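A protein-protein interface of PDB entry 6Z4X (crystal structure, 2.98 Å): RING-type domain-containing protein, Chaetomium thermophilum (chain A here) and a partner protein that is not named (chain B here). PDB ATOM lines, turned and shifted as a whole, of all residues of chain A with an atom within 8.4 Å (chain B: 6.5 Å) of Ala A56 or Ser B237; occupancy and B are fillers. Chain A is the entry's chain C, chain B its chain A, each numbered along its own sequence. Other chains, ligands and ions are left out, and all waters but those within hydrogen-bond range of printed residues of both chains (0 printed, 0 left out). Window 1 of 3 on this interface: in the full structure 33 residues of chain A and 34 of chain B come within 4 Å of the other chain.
The side-chain carboxylate (OE2) of Glu B8 is in salt-bridge range of the guanidinium group (NH1) of Arg A15 (3.999 Å).
The guanidinium group of Arg A15 lies within salt-bridge range of the side-chain carboxylate of Asp B9, at 2.9 Å.
The side-chain carboxylate (OD1) of Asp B9 is in hydrogen-bond range of the backbone NH (N) of Gly A57.
OD1 of Asp B9 sits at hydrogen-bond distance from N of Leu A58 (3.1 Å).
N of Ala A59 sits close to OD2 of Asp B9 (3.5 Å).
OG1 of Thr B235 is in hydrogen-bond range of O of Gly A57.
The side-chain hydroxyl of Thr B235 lies within hydrogen-bond range of the backbone carbonyl oxygen of Val A60 (3.5 Å).
The backbone carbonyl oxygen of Ala A56 sits at hydrogen-bond distance from the side-chain hydroxyl of Ser B237 (3.1 Å).
The side-chain hydroxyl (OG) of Ser B237 sits at hydrogen-bond distance from the backbone carbonyl oxygen (O) of Gly A57, at 3.3 Å.
The backbone NH (N) of Leu A58 is in hydrogen-bond range of the side-chain hydroxyl (OG) of Ser B237 (3.4 Å).
NE2 of Gln B238 sits at hydrogen-bond distance from O of Gly A57 (3.4 Å).
The side-chain amide nitrogen of Gln B238 sits at hydrogen-bond distance from the backbone carbonyl oxygen of Val A60 (2.5 Å).
The backbone NH (N) of Thr B235 sits at hydrogen-bond distance from the side-chain amide oxygen (OE1) of Gln B238 (3.0 Å).
The guanidinium group (NH2) of Arg A49 lies within salt-bridge range of the side-chain carboxylate (OE2) of Glu A53 (2.9 Å).
Pro A13 touches Glu B8.
Glu B8 touches Phe A52.
Ala B191 touches Glu A53 (CB to O, 3.3 Å).
CB of Ser B237 touches O of Glu A53, 3.9 Å away.
Ala A54 touches Ala B191 (CB to O, 3.2 Å).
Ala A54 touches Ser B237.
O of Ala A56 touches CG2 of Thr B235, 3.2 Å away.
Gly A57 touches Glu B8 (N to O, 3.9 Å).
Gln B238 touches Leu A58 (NE2 to O, 3.6 Å).
CD1 of Leu B241 touches CD2 of Leu A58, 3.7 Å away.
Of the printed residues of chain B, Arg A15 touches Glu B8 (3.2 Å) and Asp B9 (2.9 Å).
Ala A56 touches just these residues of chain B: Glu B8, Thr B235 and Ser B237.
Of the printed residues of chain A, Thr B235 touches Ala A56, Gly A57 and Val A60.
Of the printed residues of chain A, Met B240 touches Ala A54.
The nearest residue of chain B that does not touch Ala A56 is Asp B9 (4.1 Å).
The nearest printed residue of chain B that does not touch Leu A58 is Thr B235 (4.7 Å).
Of the 16 printed residues of chain A, 14 touch a printed residue of chain B.
Hydrophobic or aromatic side chains of chain A within 4 Å of the printed part of chain B: Phe A11, Tyr A16, Phe A52, Ala A54, Leu A58, Ala A59 and Val A60.
Among the printed residues, Asp or Glu carboxylates within 4 Å of a Lys or Arg side-chain nitrogen of the other chain: Arg A15 with Glu B8 and Arg A15 with Asp B9.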
ATOM      1  N   PHE A  11      -6.242  20.073  -9.248  1.00  0.00           N
ATOM      2  CA  PHE A  11      -7.360  19.932 -10.171  1.00  0.00           C
ATOM      3  C   PHE A  11      -7.847  18.487 -10.155  1.00  0.00           C
ATOM      4  O   PHE A  11      -7.102  17.571 -10.522  1.00  0.00           O
ATOM      5  CB  PHE A  11      -6.951  20.345 -11.584  1.00  0.00           C
ATOM      6  CG  PHE A  11      -7.965  19.991 -12.634  1.00  0.00           C
ATOM      7  CD1 PHE A  11      -9.152  20.697 -12.736  1.00  0.00           C
ATOM      8  CD2 PHE A  11      -7.733  18.954 -13.519  1.00  0.00           C
ATOM      9  CE1 PHE A  11     -10.087  20.373 -13.699  1.00  0.00           C
ATOM     10  CE2 PHE A  11      -8.665  18.625 -14.484  1.00  0.00           C
ATOM     11  CZ  PHE A  11      -9.843  19.336 -14.574  1.00  0.00           C
ATOM     12  N   PRO A  13     -11.053  16.443 -11.719  1.00  0.00           N
ATOM     13  CA  PRO A  13     -12.258  16.555 -12.548  1.00  0.00           C
ATOM     14  C   PRO A  13     -13.479  16.007 -11.828  1.00  0.00           C
ATOM     15  O   PRO A  13     -13.384  15.126 -10.969  1.00  0.00           O
ATOM     16  CB  PRO A  13     -11.914  15.720 -13.789  1.00  0.00           C
ATOM     17  CG  PRO A  13     -10.820  14.801 -13.340  1.00  0.00           C
ATOM     18  CD  PRO A  13     -10.033  15.577 -12.331  1.00  0.00           C
ATOM     19  N   ARG A  15     -16.866  15.440 -13.648  1.00  0.00           N
ATOM     20  CA  ARG A  15     -17.766  14.657 -14.481  1.00  0.00           C
ATOM     21  C   ARG A  15     -17.052  13.607 -15.321  1.00  0.00           C
ATOM     22  O   ARG A  15     -17.714  12.874 -16.063  1.00  0.00           O
ATOM     23  CB  ARG A  15     -18.572  15.588 -15.390  1.00  0.00           C
ATOM     24  CG  ARG A  15     -19.310  16.676 -14.631  1.00  0.00           C
ATOM     25  CD  ARG A  15     -20.391  17.322 -15.478  1.00  0.00           C
ATOM     26  NE  ARG A  15     -21.014  18.441 -14.778  1.00  0.00           N
ATOM     27  CZ  ARG A  15     -20.541  19.683 -14.787  1.00  0.00           C
ATOM     28  NH1 ARG A  15     -19.442  19.969 -15.472  1.00  0.00           N
ATOM     29  NH2 ARG A  15     -21.169  20.640 -14.118  1.00  0.00           N
ATOM     30  N   TYR A  16     -15.728  13.512 -15.229  1.00  0.00           N
ATOM     31  CA  TYR A  16     -14.988  12.539 -16.019  1.00  0.00           C
ATOM     32  C   TYR A  16     -13.784  12.056 -15.225  1.00  0.00           C
ATOM     33  O   TYR A  16     -13.381  12.667 -14.232  1.00  0.00           O
ATOM     34  CB  TYR A  16     -14.551  13.123 -17.369  1.00  0.00           C
ATOM     35  CG  TYR A  16     -13.411  14.117 -17.293  1.00  0.00           C
ATOM     36  CD1 TYR A  16     -13.652  15.463 -17.036  1.00  0.00           C
ATOM     37  CD2 TYR A  16     -12.096  13.716 -17.501  1.00  0.00           C
ATOM     38  CE1 TYR A  16     -12.617  16.375 -16.973  1.00  0.00           C
ATOM     39  CE2 TYR A  16     -11.053  14.622 -17.441  1.00  0.00           C
ATOM     40  CZ  TYR A  16     -11.319  15.950 -17.176  1.00  0.00           C
ATOM     41  OH  TYR A  16     -10.286  16.859 -17.115  1.00  0.00           O
ATOM     42  N   ARG A  49      -5.503  16.101 -21.692  1.00  0.00           N
ATOM     43  CA  ARG A  49      -5.890  17.372 -22.296  1.00  0.00           C
ATOM     44  C   ARG A  49      -7.163  17.222 -23.120  1.00  0.00           C
ATOM     45  O   ARG A  49      -8.067  18.064 -23.044  1.00  0.00           O
ATOM     46  CB  ARG A  49      -4.736  17.903 -23.148  1.00  0.00           C
ATOM     47  CG  ARG A  49      -4.981  19.232 -23.837  1.00  0.00           C
ATOM     48  CD  ARG A  49      -3.656  19.828 -24.297  1.00  0.00           C
ATOM     49  NE  ARG A  49      -3.787  20.682 -25.476  1.00  0.00           N
ATOM     50  CZ  ARG A  49      -4.149  21.961 -25.440  1.00  0.00           C
ATOM     51  NH1 ARG A  49      -4.232  22.661 -26.564  1.00  0.00           N
ATOM     52  NH2 ARG A  49      -4.427  22.544 -24.282  1.00  0.00           N
ATOM     53  N   ALA A  50      -7.257  16.146 -23.906  1.00  0.00           N
ATOM     54  CA  ALA A  50      -8.446  15.924 -24.722  1.00  0.00           C
ATOM     55  C   ALA A  50      -9.687  15.770 -23.852  1.00  0.00           C
ATOM     56  O   ALA A  50     -10.724  16.393 -24.112  1.00  0.00           O
ATOM     57  CB  ALA A  50      -8.251  14.693 -25.609  1.00  0.00           C
ATOM     58  N   MET A  51      -9.598  14.945 -22.807  1.00  0.00           N
ATOM     59  CA  MET A  51     -10.745  14.753 -21.923  1.00  0.00           C
ATOM     60  C   MET A  51     -11.150  16.066 -21.261  1.00  0.00           C
ATOM     61  O   MET A  51     -12.335  16.434 -21.245  1.00  0.00           O
ATOM     62  CB  MET A  51     -10.426  13.692 -20.869  1.00  0.00           C
ATOM     63  CG  MET A  51     -10.263  12.290 -21.422  1.00  0.00           C
ATOM     64  SD  MET A  51     -11.802  11.641 -22.101  1.00  0.00           S
ATOM     65  CE  MET A  51     -12.715  11.312 -20.595  1.00  0.00           C
ATOM     66  N   PHE A  52     -10.176  16.789 -20.706  1.00  0.00           N
ATOM     67  CA  PHE A  52     -10.476  18.053 -20.046  1.00  0.00           C
ATOM     68  C   PHE A  52     -11.187  19.010 -20.992  1.00  0.00           C
ATOM     69  O   PHE A  52     -12.202  19.618 -20.632  1.00  0.00           O
ATOM     70  CB  PHE A  52      -9.192  18.681 -19.508  1.00  0.00           C
ATOM     71  CG  PHE A  52      -9.383  20.060 -18.955  1.00  0.00           C
ATOM     72  CD1 PHE A  52      -9.982  20.246 -17.722  1.00  0.00           C
ATOM     73  CD2 PHE A  52      -8.966  21.171 -19.668  1.00  0.00           C
ATOM     74  CE1 PHE A  52     -10.163  21.515 -17.210  1.00  0.00           C
ATOM     75  CE2 PHE A  52      -9.142  22.444 -19.161  1.00  0.00           C
ATOM     76  CZ  PHE A  52      -9.743  22.616 -17.930  1.00  0.00           C
ATOM     77  N   GLU A  53     -10.669  19.159 -22.213  1.00  0.00           N
ATOM     78  CA  GLU A  53     -11.308  20.067 -23.160  1.00  0.00           C
ATOM     79  C   GLU A  53     -12.680  19.565 -23.588  1.00  0.00           C
ATOM     80  O   GLU A  53     -13.551  20.371 -23.934  1.00  0.00           O
ATOM     81  CB  GLU A  53     -10.405  20.282 -24.373  1.00  0.00           C
ATOM     82  CG  GLU A  53      -9.123  21.028 -24.037  1.00  0.00           C
ATOM     83  CD  GLU A  53      -8.186  21.153 -25.218  1.00  0.00           C
ATOM     84  OE1 GLU A  53      -8.562  20.713 -26.327  1.00  0.00           O
ATOM     85  OE2 GLU A  53      -7.074  21.697 -25.034  1.00  0.00           O
ATOM     86  N   ALA A  54     -12.899  18.247 -23.568  1.00  0.00           N
ATOM     87  CA  ALA A  54     -14.211  17.728 -23.936  1.00  0.00           C
ATOM     88  C   ALA A  54     -15.240  17.967 -22.839  1.00  0.00           C
ATOM     89  O   ALA A  54     -16.434  18.089 -23.131  1.00  0.00           O
ATOM     90  CB  ALA A  54     -14.117  16.237 -24.261  1.00  0.00           C
ATOM     91  N   PHE A  55     -14.807  18.044 -21.581  1.00  0.00           N
ATOM     92  CA  PHE A  55     -15.738  18.240 -20.477  1.00  0.00           C
ATOM     93  C   PHE A  55     -15.614  19.595 -19.793  1.00  0.00           C
ATOM     94  O   PHE A  55     -16.465  19.922 -18.958  1.00  0.00           O
ATOM     95  CB  PHE A  55     -15.562  17.133 -19.428  1.00  0.00           C
ATOM     96  CG  PHE A  55     -16.048  15.789 -19.884  1.00  0.00           C
ATOM     97  CD1 PHE A  55     -15.221  14.953 -20.613  1.00  0.00           C
ATOM     98  CD2 PHE A  55     -17.334  15.364 -19.592  1.00  0.00           C
ATOM     99  CE1 PHE A  55     -15.662  13.718 -21.039  1.00  0.00           C
ATOM    100  CE2 PHE A  55     -17.782  14.127 -20.017  1.00  0.00           C
ATOM    101  CZ  PHE A  55     -16.944  13.304 -20.741  1.00  0.00           C
ATOM    102  N   ALA A  56     -14.595  20.388 -20.118  1.00  0.00           N
ATOM    103  CA  ALA A  56     -14.420  21.688 -19.477  1.00  0.00           C
ATOM    104  C   ALA A  56     -15.515  22.650 -19.925  1.00  0.00           C
ATOM    105  O   ALA A  56     -15.655  22.935 -21.120  1.00  0.00           O
ATOM    106  CB  ALA A  56     -13.040  22.255 -19.798  1.00  0.00           C
ATOM    107  N   GLY A  57     -16.282  23.162 -18.966  1.00  0.00           N
ATOM    108  CA  GLY A  57     -17.342  24.098 -19.282  1.00  0.00           C
ATOM    109  C   GLY A  57     -18.600  23.465 -19.828  1.00  0.00           C
ATOM    110  O   GLY A  57     -19.338  24.115 -20.573  1.00  0.00           O
ATOM    111  N   LEU A  58     -18.874  22.207 -19.472  1.00  0.00           N
ATOM    112  CA  LEU A  58     -20.067  21.547 -19.993  1.00  0.00           C
ATOM    113  C   LEU A  58     -21.338  22.189 -19.452  1.00  0.00           C
ATOM    114  O   LEU A  58     -22.348  22.256 -20.163  1.00  0.00           O
ATOM    115  CB  LEU A  58     -20.037  20.054 -19.659  1.00  0.00           C
ATOM    116  CG  LEU A  58     -20.608  19.118 -20.731  1.00  0.00           C
ATOM    117  CD1 LEU A  58     -20.587  17.674 -20.253  1.00  0.00           C
ATOM    118  CD2 LEU A  58     -22.015  19.533 -21.135  1.00  0.00           C
ATOM    119  N   ALA A  59     -21.312  22.657 -18.203  1.00  0.00           N
ATOM    120  CA  ALA A  59     -22.456  23.303 -17.577  1.00  0.00           C
ATOM    121  C   ALA A  59     -22.303  24.819 -17.504  1.00  0.00           C
ATOM    122  O   ALA A  59     -22.954  25.464 -16.676  1.00  0.00           O
ATOM    123  CB  ALA A  59     -22.690  22.728 -16.179  1.00  0.00           C
ATOM    124  N   VAL A  60     -21.460  25.400 -18.357  1.00  0.00           N
ATOM    125  CA  VAL A  60     -21.264  26.846 -18.400  1.00  0.00           C
ATOM    126  C   VAL A  60     -22.271  27.406 -19.400  1.00  0.00           C
ATOM    127  O   VAL A  60     -22.078  27.320 -20.613  1.00  0.00           O
ATOM    128  CB  VAL A  60     -19.828  27.214 -18.770  1.00  0.00           C
ATOM    129  CG1 VAL A  60     -19.716  28.711 -19.031  1.00  0.00           C
ATOM    130  CG2 VAL A  60     -18.872  26.794 -17.665  1.00  0.00           C
ATOM    131  N   GLU B   8     -13.821  21.751 -13.558  1.00  0.00           N
ATOM    132  CA  GLU B   8     -13.485  22.091 -14.936  1.00  0.00           C
ATOM    133  C   GLU B   8     -14.284  23.297 -15.414  1.00  0.00           C
ATOM    134  O   GLU B   8     -13.759  24.147 -16.145  1.00  0.00           O
ATOM    135  CB  GLU B   8     -13.726  20.886 -15.848  1.00  0.00           C
ATOM    136  CG  GLU B   8     -15.130  20.293 -15.777  1.00  0.00           C
ATOM    137  CD  GLU B   8     -15.238  19.138 -14.795  1.00  0.00           C
ATOM    138  OE1 GLU B   8     -14.655  19.230 -13.693  1.00  0.00           O
ATOM    139  OE2 GLU B   8     -15.905  18.134 -15.130  1.00  0.00           O
ATOM    140  N   ASP B   9     -15.544  23.404 -14.991  1.00  0.00           N
ATOM    141  CA  ASP B   9     -16.350  24.564 -15.356  1.00  0.00           C
ATOM    142  C   ASP B   9     -15.752  25.849 -14.794  1.00  0.00           C
ATOM    143  O   ASP B   9     -15.719  26.877 -15.479  1.00  0.00           O
ATOM    144  CB  ASP B   9     -17.786  24.371 -14.867  1.00  0.00           C
ATOM    145  CG  ASP B   9     -18.502  23.247 -15.594  1.00  0.00           C
ATOM    146  OD1 ASP B   9     -17.932  22.713 -16.570  1.00  0.00           O
ATOM    147  OD2 ASP B   9     -19.632  22.898 -15.190  1.00  0.00           O
ATOM    148  N   ARG B  11     -12.500  26.328 -13.991  1.00  0.00           N
ATOM    149  CA  ARG B  11     -11.252  26.603 -14.696  1.00  0.00           C
ATOM    150  C   ARG B  11     -11.511  27.153 -16.094  1.00  0.00           C
ATOM    151  O   ARG B  11     -10.704  27.932 -16.612  1.00  0.00           O
ATOM    152  CB  ARG B  11     -10.381  25.344 -14.750  1.00  0.00           C
ATOM    153  CG  ARG B  11      -8.970  25.589 -15.289  1.00  0.00           C
ATOM    154  CD  ARG B  11      -7.913  24.800 -14.508  1.00  0.00           C
ATOM    155  NE  ARG B  11      -7.807  23.395 -14.901  1.00  0.00           N
ATOM    156  CZ  ARG B  11      -6.794  22.887 -15.598  1.00  0.00           C
ATOM    157  NH1 ARG B  11      -6.779  21.597 -15.903  1.00  0.00           N
ATOM    158  NH2 ARG B  11      -5.794  23.665 -15.988  1.00  0.00           N
ATOM    159  N   TYR B  12     -12.630  26.773 -16.718  1.00  0.00           N
ATOM    160  CA  TYR B  12     -12.986  27.382 -17.998  1.00  0.00           C
ATOM    161  C   TYR B  12     -13.489  28.810 -17.813  1.00  0.00           C
ATOM    162  O   TYR B  12     -13.151  29.699 -18.602  1.00  0.00           O
ATOM    163  CB  TYR B  12     -14.035  26.541 -18.724  1.00  0.00           C
ATOM    164  CG  TYR B  12     -14.472  27.143 -20.044  1.00  0.00           C
ATOM    165  CD1 TYR B  12     -13.753  26.915 -21.210  1.00  0.00           C
ATOM    166  CD2 TYR B  12     -15.599  27.948 -20.119  1.00  0.00           C
ATOM    167  CE1 TYR B  12     -14.148  27.469 -22.415  1.00  0.00           C
ATOM    168  CE2 TYR B  12     -16.002  28.505 -21.320  1.00  0.00           C
ATOM    169  CZ  TYR B  12     -15.274  28.262 -22.464  1.00  0.00           C
ATOM    170  OH  TYR B  12     -15.672  28.815 -23.660  1.00  0.00           O
ATOM    171  N   PRO B 188     -12.712  23.005 -30.171  1.00  0.00           N
ATOM    172  CA  PRO B 188     -13.320  21.718 -29.779  1.00  0.00           C
ATOM    173  C   PRO B 188     -12.849  20.499 -30.566  1.00  0.00           C
ATOM    174  O   PRO B 188     -13.476  19.442 -30.436  1.00  0.00           O
ATOM    175  CB  PRO B 188     -14.811  21.977 -30.044  1.00  0.00           C
ATOM    176  CG  PRO B 188     -14.887  23.272 -30.878  1.00  0.00           C
ATOM    177  CD  PRO B 188     -13.490  23.666 -31.224  1.00  0.00           C
ATOM    178  N   ALA B 191     -11.306  18.169 -28.060  1.00  0.00           N
ATOM    179  CA  ALA B 191     -12.444  17.740 -27.256  1.00  0.00           C
ATOM    180  C   ALA B 191     -13.264  16.687 -27.989  1.00  0.00           C
ATOM    181  O   ALA B 191     -13.760  15.735 -27.375  1.00  0.00           O
ATOM    182  CB  ALA B 191     -13.312  18.941 -26.886  1.00  0.00           C
ATOM    183  N   PHE B 234     -21.388  29.634 -26.687  1.00  0.00           N
ATOM    184  CA  PHE B 234     -21.257  28.255 -26.247  1.00  0.00           C
ATOM    185  C   PHE B 234     -19.798  27.952 -25.938  1.00  0.00           C
ATOM    186  O   PHE B 234     -18.882  28.607 -26.439  1.00  0.00           O
ATOM    187  CB  PHE B 234     -21.796  27.277 -27.298  1.00  0.00           C
ATOM    188  CG  PHE B 234     -23.217  27.544 -27.693  1.00  0.00           C
ATOM    189  CD1 PHE B 234     -24.262  27.093 -26.905  1.00  0.00           C
ATOM    190  CD2 PHE B 234     -23.512  28.255 -28.844  1.00  0.00           C
ATOM    191  CE1 PHE B 234     -25.573  27.339 -27.260  1.00  0.00           C
ATOM    192  CE2 PHE B 234     -24.822  28.505 -29.205  1.00  0.00           C
ATOM    193  CZ  PHE B 234     -25.853  28.045 -28.411  1.00  0.00           C
ATOM    194  N   THR B 235     -19.602  26.948 -25.097  1.00  0.00           N
ATOM    195  CA  THR B 235     -18.347  26.405 -24.606  1.00  0.00           C
ATOM    196  C   THR B 235     -17.788  25.386 -25.594  1.00  0.00           C
ATOM    197  O   THR B 235     -18.549  24.679 -26.261  1.00  0.00           O
ATOM    198  CB  THR B 235     -18.557  25.735 -23.252  1.00  0.00           C
ATOM    199  OG1 THR B 235     -19.151  26.672 -22.345  1.00  0.00           O
ATOM    200  CG2 THR B 235     -17.231  25.255 -22.680  1.00  0.00           C
ATOM    201  N   PRO B 236     -16.459  25.300 -25.713  1.00  0.00           N
ATOM    202  CA  PRO B 236     -15.874  24.284 -26.603  1.00  0.00           C
ATOM    203  C   PRO B 236     -16.477  22.904 -26.416  1.00  0.00           C
ATOM    204  O   PRO B 236     -16.730  22.206 -27.405  1.00  0.00           O
ATOM    205  CB  PRO B 236     -14.387  24.322 -26.230  1.00  0.00           C
ATOM    206  CG  PRO B 236     -14.162  25.736 -25.828  1.00  0.00           C
ATOM    207  CD  PRO B 236     -15.431  26.187 -25.141  1.00  0.00           C
ATOM    208  N   SER B 237     -16.723  22.489 -25.171  1.00  0.00           N
ATOM    209  CA  SER B 237     -17.389  21.210 -24.947  1.00  0.00           C
ATOM    210  C   SER B 237     -18.801  21.226 -25.515  1.00  0.00           C
ATOM    211  O   SER B 237     -19.242  20.251 -26.134  1.00  0.00           O
ATOM    212  CB  SER B 237     -17.409  20.879 -23.455  1.00  0.00           C
ATOM    213  OG  SER B 237     -18.126  21.859 -22.727  1.00  0.00           O
ATOM    214  N   GLN B 238     -19.525  22.329 -25.320  1.00  0.00           N
ATOM    215  CA  GLN B 238     -20.882  22.422 -25.849  1.00  0.00           C
ATOM    216  C   GLN B 238     -20.885  22.395 -27.372  1.00  0.00           C
ATOM    217  O   GLN B 238     -21.719  21.721 -27.988  1.00  0.00           O
ATOM    218  CB  GLN B 238     -21.555  23.692 -25.333  1.00  0.00           C
ATOM    219  CG  GLN B 238     -21.653  23.767 -23.822  1.00  0.00           C
ATOM    220  CD  GLN B 238     -22.065  25.140 -23.332  1.00  0.00           C
ATOM    221  OE1 GLN B 238     -22.287  26.056 -24.126  1.00  0.00           O
ATOM    222  NE2 GLN B 238     -22.162  25.292 -22.017  1.00  0.00           N
ATOM    223  N   ILE B 239     -19.952  23.116 -27.997  1.00  0.00           N
ATOM    224  CA  ILE B 239     -19.876  23.128 -29.454  1.00  0.00           C
ATOM    225  C   ILE B 239     -19.493  21.750 -29.986  1.00  0.00           C
ATOM    226  O   ILE B 239     -20.013  21.300 -31.015  1.00  0.00           O
ATOM    227  CB  ILE B 239     -18.901  24.223 -29.923  1.00  0.00           C
ATOM    228  CG1 ILE B 239     -19.427  25.603 -29.517  1.00  0.00           C
ATOM    229  CG2 ILE B 239     -18.690  24.144 -31.426  1.00  0.00           C
ATOM    230  CD1 ILE B 239     -18.483  26.741 -29.825  1.00  0.00           C
ATOM    231  N   MET B 240     -18.570  21.065 -29.305  1.00  0.00           N
ATOM    232  CA  MET B 240     -18.193  19.716 -29.714  1.00  0.00           C
ATOM    233  C   MET B 240     -19.381  18.766 -29.614  1.00  0.00           C
ATOM    234  O   MET B 240     -19.629  17.962 -30.523  1.00  0.00           O
ATOM    235  CB  MET B 240     -17.025  19.215 -28.863  1.00  0.00           C
ATOM    236  CG  MET B 240     -16.608  17.779 -29.159  1.00  0.00           C
ATOM    237  SD  MET B 240     -17.556  16.523 -28.271  1.00  0.00           S
ATOM    238  CE  MET B 240     -17.128  16.901 -26.573  1.00  0.00           C
ATOM    239  N   LEU B 241     -20.120  18.832 -28.503  1.00  0.00           N
ATOM    240  CA  LEU B 241     -21.300  17.987 -28.352  1.00  0.00           C
ATOM    241  C   LEU B 241     -22.358  18.314 -29.397  1.00  0.00           C
ATOM    242  O   LEU B 241     -23.055  17.413 -29.872  1.00  0.00           O
ATOM    243  CB  LEU B 241     -21.873  18.128 -26.942  1.00  0.00           C
ATOM    244  CG  LEU B 241     -21.012  17.508 -25.841  1.00  0.00           C
ATOM    245  CD1 LEU B 241     -21.538  17.889 -24.468  1.00  0.00           C
ATOM    246  CD2 LEU B 241     -20.964  15.998 -26.005  1.00  0.00           C
ATOM    247  N   ALA B 242     -22.477  19.584 -29.784  1.00  0.00           N
ATOM    248  CA  ALA B 242     -23.423  19.946 -30.832  1.00  0.00           C
ATOM    249  C   ALA B 242     -23.001  19.368 -32.178  1.00  0.00           C
ATOM    250  O   ALA B 242     -23.832  18.829 -32.918  1.00  0.00           O
ATOM    251  CB  ALA B 242     -23.558  21.465 -30.918  1.00  0.00           C
ATOM    252  N   ILE B 322     -27.170  22.424 -25.740  1.00  0.00           N
ATOM    253  CA  ILE B 322     -26.622  21.638 -26.840  1.00  0.00           C
ATOM    254  C   ILE B 322     -27.540  21.704 -28.051  1.00  0.00           C
ATOM    255  O   ILE B 322     -27.077  21.794 -29.192  1.00  0.00           O
ATOM    256  CB  ILE B 322     -26.385  20.184 -26.388  1.00  0.00           C
ATOM    257  CG1 ILE B 322     -25.375  20.141 -25.239  1.00  0.00           C
ATOM    258  CG2 ILE B 322     -25.917  19.332 -27.555  1.00  0.00           C
ATOM    259  CD1 ILE B 322     -24.022  20.714 -25.592  1.00  0.00           C
